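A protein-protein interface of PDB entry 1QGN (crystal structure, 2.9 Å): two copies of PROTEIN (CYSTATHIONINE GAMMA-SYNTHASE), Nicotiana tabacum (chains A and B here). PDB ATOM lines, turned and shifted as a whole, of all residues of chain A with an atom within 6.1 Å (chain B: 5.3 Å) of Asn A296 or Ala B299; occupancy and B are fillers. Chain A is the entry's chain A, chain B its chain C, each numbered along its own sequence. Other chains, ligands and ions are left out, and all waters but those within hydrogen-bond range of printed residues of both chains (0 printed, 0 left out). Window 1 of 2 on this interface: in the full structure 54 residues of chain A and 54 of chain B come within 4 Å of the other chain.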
ATOM      1  N   VAL A  81     -21.620   7.555 -16.937  1.00  0.00           N
ATOM      2  CA  VAL A  81     -20.310   8.185 -16.854  1.00  0.00           C
ATOM      3  C   VAL A  81     -20.220   9.149 -18.032  1.00  0.00           C
ATOM      4  O   VAL A  81     -20.264   8.738 -19.187  1.00  0.00           O
ATOM      5  CB  VAL A  81     -19.183   7.160 -16.975  1.00  0.00           C
ATOM      6  CG1 VAL A  81     -17.864   7.809 -16.604  1.00  0.00           C
ATOM      7  CG2 VAL A  81     -19.464   5.970 -16.083  1.00  0.00           C
ATOM      8  N   ASN A  83     -17.949  11.391 -20.018  1.00  0.00           N
ATOM      9  CA  ASN A  83     -16.567  11.727 -20.373  1.00  0.00           C
ATOM     10  C   ASN A  83     -16.483  12.925 -21.312  1.00  0.00           C
ATOM     11  O   ASN A  83     -16.349  12.753 -22.518  1.00  0.00           O
ATOM     12  CB  ASN A  83     -15.913  10.536 -21.068  1.00  0.00           C
ATOM     13  CG  ASN A  83     -15.324   9.544 -20.095  1.00  0.00           C
ATOM     14  OD1 ASN A  83     -14.350   9.842 -19.385  1.00  0.00           O
ATOM     15  ND2 ASN A  83     -15.901   8.345 -20.062  1.00  0.00           N
ATOM     16  N   THR A 116     -20.532  13.335 -11.548  1.00  0.00           N
ATOM     17  CA  THR A 116     -19.837  13.619 -10.291  1.00  0.00           C
ATOM     18  C   THR A 116     -20.742  14.271  -9.241  1.00  0.00           C
ATOM     19  O   THR A 116     -20.622  13.959  -8.055  1.00  0.00           O
ATOM     20  CB  THR A 116     -18.581  14.502 -10.528  1.00  0.00           C
ATOM     21  OG1 THR A 116     -17.498  13.671 -10.951  1.00  0.00           O
ATOM     22  CG2 THR A 116     -18.156  15.212  -9.262  1.00  0.00           C
ATOM     23  N   ALA A 294      -9.280  18.442 -10.123  1.00  0.00           N
ATOM     24  CA  ALA A 294     -10.535  17.769 -10.454  1.00  0.00           C
ATOM     25  C   ALA A 294     -10.530  16.253 -10.379  1.00  0.00           C
ATOM     26  O   ALA A 294      -9.484  15.617 -10.468  1.00  0.00           O
ATOM     27  CB  ALA A 294     -10.989  18.199 -11.830  1.00  0.00           C
ATOM     28  N   LEU A 295     -11.723  15.684 -10.226  1.00  0.00           N
ATOM     29  CA  LEU A 295     -11.900  14.237 -10.140  1.00  0.00           C
ATOM     30  C   LEU A 295     -12.475  13.701 -11.448  1.00  0.00           C
ATOM     31  O   LEU A 295     -13.448  14.232 -11.978  1.00  0.00           O
ATOM     32  CB  LEU A 295     -12.836  13.895  -8.973  1.00  0.00           C
ATOM     33  CG  LEU A 295     -13.286  12.441  -8.792  1.00  0.00           C
ATOM     34  CD1 LEU A 295     -12.356  11.735  -7.827  1.00  0.00           C
ATOM     35  CD2 LEU A 295     -14.718  12.407  -8.271  1.00  0.00           C
ATOM     36  N   ASN A 296     -11.873  12.643 -11.967  1.00  0.00           N
ATOM     37  CA  ASN A 296     -12.329  12.058 -13.218  1.00  0.00           C
ATOM     38  C   ASN A 296     -13.657  11.335 -13.039  1.00  0.00           C
ATOM     39  O   ASN A 296     -13.869  10.639 -12.048  1.00  0.00           O
ATOM     40  CB  ASN A 296     -11.279  11.079 -13.750  1.00  0.00           C
ATOM     41  CG  ASN A 296     -11.637  10.521 -15.108  1.00  0.00           C
ATOM     42  OD1 ASN A 296     -12.238   9.455 -15.217  1.00  0.00           O
ATOM     43  ND2 ASN A 296     -11.268  11.243 -16.160  1.00  0.00           N
ATOM     44  N   PRO A 297     -14.567  11.486 -14.005  1.00  0.00           N
ATOM     45  CA  PRO A 297     -15.879  10.842 -13.951  1.00  0.00           C
ATOM     46  C   PRO A 297     -15.789   9.342 -13.724  1.00  0.00           C
ATOM     47  O   PRO A 297     -16.636   8.765 -13.050  1.00  0.00           O
ATOM     48  CB  PRO A 297     -16.502  11.171 -15.305  1.00  0.00           C
ATOM     49  CG  PRO A 297     -15.827  12.415 -15.734  1.00  0.00           C
ATOM     50  CD  PRO A 297     -14.412  12.292 -15.228  1.00  0.00           C
ATOM     51  N   ASN A 298     -14.773   8.708 -14.293  1.00  0.00           N
ATOM     52  CA  ASN A 298     -14.613   7.273 -14.130  1.00  0.00           C
ATOM     53  C   ASN A 298     -14.305   6.940 -12.685  1.00  0.00           C
ATOM     54  O   ASN A 298     -14.625   5.851 -12.213  1.00  0.00           O
ATOM     55  CB  ASN A 298     -13.491   6.760 -15.022  1.00  0.00           C
ATOM     56  CG  ASN A 298     -13.795   6.943 -16.480  1.00  0.00           C
ATOM     57  OD1 ASN A 298     -14.687   6.294 -17.019  1.00  0.00           O
ATOM     58  ND2 ASN A 298     -13.059   7.835 -17.133  1.00  0.00           N
ATOM     59  N   ALA A 299     -13.668   7.876 -11.988  1.00  0.00           N
ATOM     60  CA  ALA A 299     -13.328   7.675 -10.586  1.00  0.00           C
ATOM     61  C   ALA A 299     -14.601   7.906  -9.775  1.00  0.00           C
ATOM     62  O   ALA A 299     -14.933   7.131  -8.873  1.00  0.00           O
ATOM     63  CB  ALA A 299     -12.256   8.647 -10.167  1.00  0.00           C
ATOM     64  N   ALA A 300     -15.324   8.967 -10.108  1.00  0.00           N
ATOM     65  CA  ALA A 300     -16.558   9.269  -9.412  1.00  0.00           C
ATOM     66  C   ALA A 300     -17.514   8.078  -9.484  1.00  0.00           C
ATOM     67  O   ALA A 300     -18.253   7.808  -8.538  1.00  0.00           O
ATOM     68  CB  ALA A 300     -17.206  10.492 -10.018  1.00  0.00           C
ATOM     69  N   TYR A 301     -17.500   7.352 -10.594  1.00  0.00           N
ATOM     70  CA  TYR A 301     -18.399   6.213 -10.729  1.00  0.00           C
ATOM     71  C   TYR A 301     -17.946   5.020  -9.907  1.00  0.00           C
ATOM     72  O   TYR A 301     -18.765   4.346  -9.289  1.00  0.00           O
ATOM     73  CB  TYR A 301     -18.543   5.797 -12.198  1.00  0.00           C
ATOM     74  CG  TYR A 301     -19.486   4.637 -12.392  1.00  0.00           C
ATOM     75  CD1 TYR A 301     -20.866   4.828 -12.401  1.00  0.00           C
ATOM     76  CD2 TYR A 301     -19.002   3.338 -12.510  1.00  0.00           C
ATOM     77  CE1 TYR A 301     -21.749   3.739 -12.515  1.00  0.00           C
ATOM     78  CE2 TYR A 301     -19.869   2.245 -12.625  1.00  0.00           C
ATOM     79  CZ  TYR A 301     -21.243   2.451 -12.621  1.00  0.00           C
ATOM     80  OH  TYR A 301     -22.098   1.365 -12.679  1.00  0.00           O
ATOM     81  N   VAL B 269     -11.497  14.398 -21.665  1.00  0.00           N
ATOM     82  CA  VAL B 269     -10.619  14.197 -20.509  1.00  0.00           C
ATOM     83  C   VAL B 269      -9.742  15.413 -20.180  1.00  0.00           C
ATOM     84  O   VAL B 269      -9.268  16.112 -21.082  1.00  0.00           O
ATOM     85  CB  VAL B 269      -9.706  12.965 -20.731  1.00  0.00           C
ATOM     86  CG1 VAL B 269      -8.878  13.160 -21.980  1.00  0.00           C
ATOM     87  CG2 VAL B 269      -8.796  12.751 -19.533  1.00  0.00           C
ATOM     88  N   LEU B 270      -9.535  15.669 -18.888  1.00  0.00           N
ATOM     89  CA  LEU B 270      -8.695  16.787 -18.455  1.00  0.00           C
ATOM     90  C   LEU B 270      -7.355  16.256 -17.986  1.00  0.00           C
ATOM     91  O   LEU B 270      -7.280  15.159 -17.438  1.00  0.00           O
ATOM     92  CB  LEU B 270      -9.331  17.548 -17.295  1.00  0.00           C
ATOM     93  CG  LEU B 270     -10.741  18.116 -17.411  1.00  0.00           C
ATOM     94  CD1 LEU B 270     -10.744  19.514 -16.841  1.00  0.00           C
ATOM     95  CD2 LEU B 270     -11.203  18.125 -18.846  1.00  0.00           C
ATOM     96  N   LEU B 295      -3.453  12.004 -11.340  1.00  0.00           N
ATOM     97  CA  LEU B 295      -4.219  11.731 -12.550  1.00  0.00           C
ATOM     98  C   LEU B 295      -4.706  10.292 -12.494  1.00  0.00           C
ATOM     99  O   LEU B 295      -3.938   9.392 -12.176  1.00  0.00           O
ATOM    100  CB  LEU B 295      -3.337  11.937 -13.785  1.00  0.00           C
ATOM    101  CG  LEU B 295      -3.914  11.523 -15.142  1.00  0.00           C
ATOM    102  CD1 LEU B 295      -4.596  12.715 -15.797  1.00  0.00           C
ATOM    103  CD2 LEU B 295      -2.805  10.989 -16.027  1.00  0.00           C
ATOM    104  N   ASN B 296      -5.982  10.073 -12.797  1.00  0.00           N
ATOM    105  CA  ASN B 296      -6.550   8.725 -12.759  1.00  0.00           C
ATOM    106  C   ASN B 296      -6.060   7.892 -13.940  1.00  0.00           C
ATOM    107  O   ASN B 296      -5.947   8.391 -15.055  1.00  0.00           O
ATOM    108  CB  ASN B 296      -8.080   8.806 -12.765  1.00  0.00           C
ATOM    109  CG  ASN B 296      -8.732   7.456 -12.620  1.00  0.00           C
ATOM    110  OD1 ASN B 296      -9.096   6.831 -13.608  1.00  0.00           O
ATOM    111  ND2 ASN B 296      -8.887   6.996 -11.383  1.00  0.00           N
ATOM    112  N   PRO B 297      -5.764   6.607 -13.713  1.00  0.00           N
ATOM    113  CA  PRO B 297      -5.281   5.703 -14.759  1.00  0.00           C
ATOM    114  C   PRO B 297      -6.172   5.654 -15.983  1.00  0.00           C
ATOM    115  O   PRO B 297      -5.693   5.493 -17.102  1.00  0.00           O
ATOM    116  CB  PRO B 297      -5.214   4.350 -14.061  1.00  0.00           C
ATOM    117  CG  PRO B 297      -5.035   4.684 -12.643  1.00  0.00           C
ATOM    118  CD  PRO B 297      -5.872   5.915 -12.424  1.00  0.00           C
ATOM    119  N   ASN B 298      -7.474   5.767 -15.765  1.00  0.00           N
ATOM    120  CA  ASN B 298      -8.417   5.751 -16.869  1.00  0.00           C
ATOM    121  C   ASN B 298      -8.217   6.991 -17.728  1.00  0.00           C
ATOM    122  O   ASN B 298      -8.416   6.945 -18.934  1.00  0.00           O
ATOM    123  CB  ASN B 298      -9.847   5.701 -16.334  1.00  0.00           C
ATOM    124  CG  ASN B 298     -10.117   4.442 -15.551  1.00  0.00           C
ATOM    125  OD1 ASN B 298     -10.105   3.348 -16.105  1.00  0.00           O
ATOM    126  ND2 ASN B 298     -10.348   4.584 -14.256  1.00  0.00           N
ATOM    127  N   ALA B 299      -7.822   8.100 -17.112  1.00  0.00           N
ATOM    128  CA  ALA B 299      -7.598   9.323 -17.858  1.00  0.00           C
ATOM    129  C   ALA B 299      -6.303   9.151 -18.626  1.00  0.00           C
ATOM    130  O   ALA B 299      -6.222   9.440 -19.818  1.00  0.00           O
ATOM    131  CB  ALA B 299      -7.495  10.506 -16.918  1.00  0.00           C
ATOM    132  N   ALA B 300      -5.284   8.664 -17.934  1.00  0.00           N
ATOM    133  CA  ALA B 300      -3.991   8.447 -18.555  1.00  0.00           C
ATOM    134  C   ALA B 300      -4.149   7.605 -19.819  1.00  0.00           C
ATOM    135  O   ALA B 300      -3.480   7.846 -20.820  1.00  0.00           O
ATOM    136  CB  ALA B 300      -3.046   7.754 -17.574  1.00  0.00           C
ATOM    137  N   TYR B 301      -5.039   6.624 -19.786  1.00  0.00           N
ATOM    138  CA  TYR B 301      -5.220   5.771 -20.950  1.00  0.00           C
ATOM    139  C   TYR B 301      -5.944   6.476 -22.080  1.00  0.00           C
ATOM    140  O   TYR B 301      -5.593   6.306 -23.242  1.00  0.00           O
ATOM    141  CB  TYR B 301      -5.981   4.497 -20.580  1.00  0.00           C
ATOM    142  CG  TYR B 301      -6.154   3.573 -21.756  1.00  0.00           C
ATOM    143  CD1 TYR B 301      -5.117   2.748 -22.171  1.00  0.00           C
ATOM    144  CD2 TYR B 301      -7.340   3.564 -22.491  1.00  0.00           C
ATOM    145  CE1 TYR B 301      -5.251   1.936 -23.295  1.00  0.00           C
ATOM    146  CE2 TYR B 301      -7.488   2.751 -23.623  1.00  0.00           C
ATOM    147  CZ  TYR B 301      -6.432   1.942 -24.019  1.00  0.00           C
ATOM    148  OH  TYR B 301      -6.533   1.166 -25.156  1.00  0.00           O
ATOM    149  N   LEU B 302      -6.960   7.263 -21.745  1.00  0.00           N
ATOM    150  CA  LEU B 302      -7.713   7.975 -22.769  1.00  0.00           C
ATOM    151  C   LEU B 302      -6.795   8.902 -23.549  1.00  0.00           C
ATOM    152  O   LEU B 302      -7.014   9.152 -24.735  1.00  0.00           O
ATOM    153  CB  LEU B 302      -8.851   8.774 -22.141  1.00  0.00           C
ATOM    154  CG  LEU B 302     -10.131   7.963 -21.891  1.00  0.00           C
ATOM    155  CD1 LEU B 302     -11.254   8.901 -21.452  1.00  0.00           C
ATOM    156  CD2 LEU B 302     -10.530   7.200 -23.156  1.00  0.00           C
ATOM    157  N   ILE B 303      -5.765   9.401 -22.874  1.00  0.00           N
ATOM    158  CA  ILE B 303      -4.802  10.295 -23.498  1.00  0.00           C
ATOM    159  C   ILE B 303      -3.772   9.483 -24.283  1.00  0.00           C
ATOM    160  O   ILE B 303      -3.428   9.826 -25.411  1.00  0.00           O
ATOM    161  CB  ILE B 303      -4.091  11.150 -22.442  1.00  0.00           C
ATOM    162  CG1 ILE B 303      -5.043  12.235 -21.941  1.00  0.00           C
ATOM    163  CG2 ILE B 303      -2.829  11.778 -23.030  1.00  0.00           C
ATOM    164  CD1 ILE B 303      -4.512  12.993 -20.755  1.00  0.00           C
ATOM    165  N   ILE B 304      -3.275   8.410 -23.683  1.00  0.00           N
ATOM    166  CA  ILE B 304      -2.305   7.552 -24.356  1.00  0.00           C
ATOM    167  C   ILE B 304      -2.920   7.163 -25.699  1.00  0.00           C
ATOM    168  O   ILE B 304      -2.274   7.235 -26.745  1.00  0.00           O
ATOM    169  CB  ILE B 304      -2.025   6.276 -23.520  1.00  0.00           C
ATOM    170  CG1 ILE B 304      -1.092   6.616 -22.358  1.00  0.00           C
ATOM    171  CG2 ILE B 304      -1.420   5.194 -24.388  1.00  0.00           C
ATOM    172  CD1 ILE B 304      -0.631   5.415 -21.571  1.00  0.00           C
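Asn A296 touches just one residue of chain B: Ala B299.
Of the printed residues of chain A, Leu B302 touches Asn A83 (3.8 Å).
Of the printed residues of chain A, Asn B298 touches Asn A298 (3.9 Å).
Of the printed residues of chain B, Asn A83 touches Leu B302.
Of the printed residues of chain B, Asn A298 touches Asn B298 (3.9 Å).
Val A81 touches none of the printed residues of chain B.
The nearest residue of chain A that does not touch Ala B299 is Asn A298 (5.2 Å).
The nearest printed residue of chain B that does not touch Ala A299 is Asn B298 (5.2 Å).
The side-chain amide oxygen of Asn A83 is in hydrogen-bond range of the side-chain amide nitrogen of Asn A298 (3.3 Å).
OD1 of Asn A296 is in hydrogen-bond range of ND2 of Asn A298.
The side-chain amide oxygen (OD1) of Asn B296 lies within hydrogen-bond range of the side-chain amide nitrogen (ND2) of Asn B298 (2.7 Å).
Among the printed residues, merely in contact across the chains: Asn A83 with Leu B302, Asn A298 with Asn B298, Asn A296 with Ala B299 and Ala A299 with Asn B296.
Asn A296 touches Ala B299, and with the chains exchanged Ala A299 touches Asn B296.
Asn A298 touches its own counterpart, Asn B298.
Of the 11 printed residues of chain A, 4 touch a printed residue of chain B.
Printed residues of chain A that touch a printed residue of chain B: Asn A83, Asn A296, Asn A298 and Ala A299.
Among the printed residues, no Asp or Glu carboxylate lies within 4 Å of a Lys or Arg side-chain nitrogen of the other chain.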
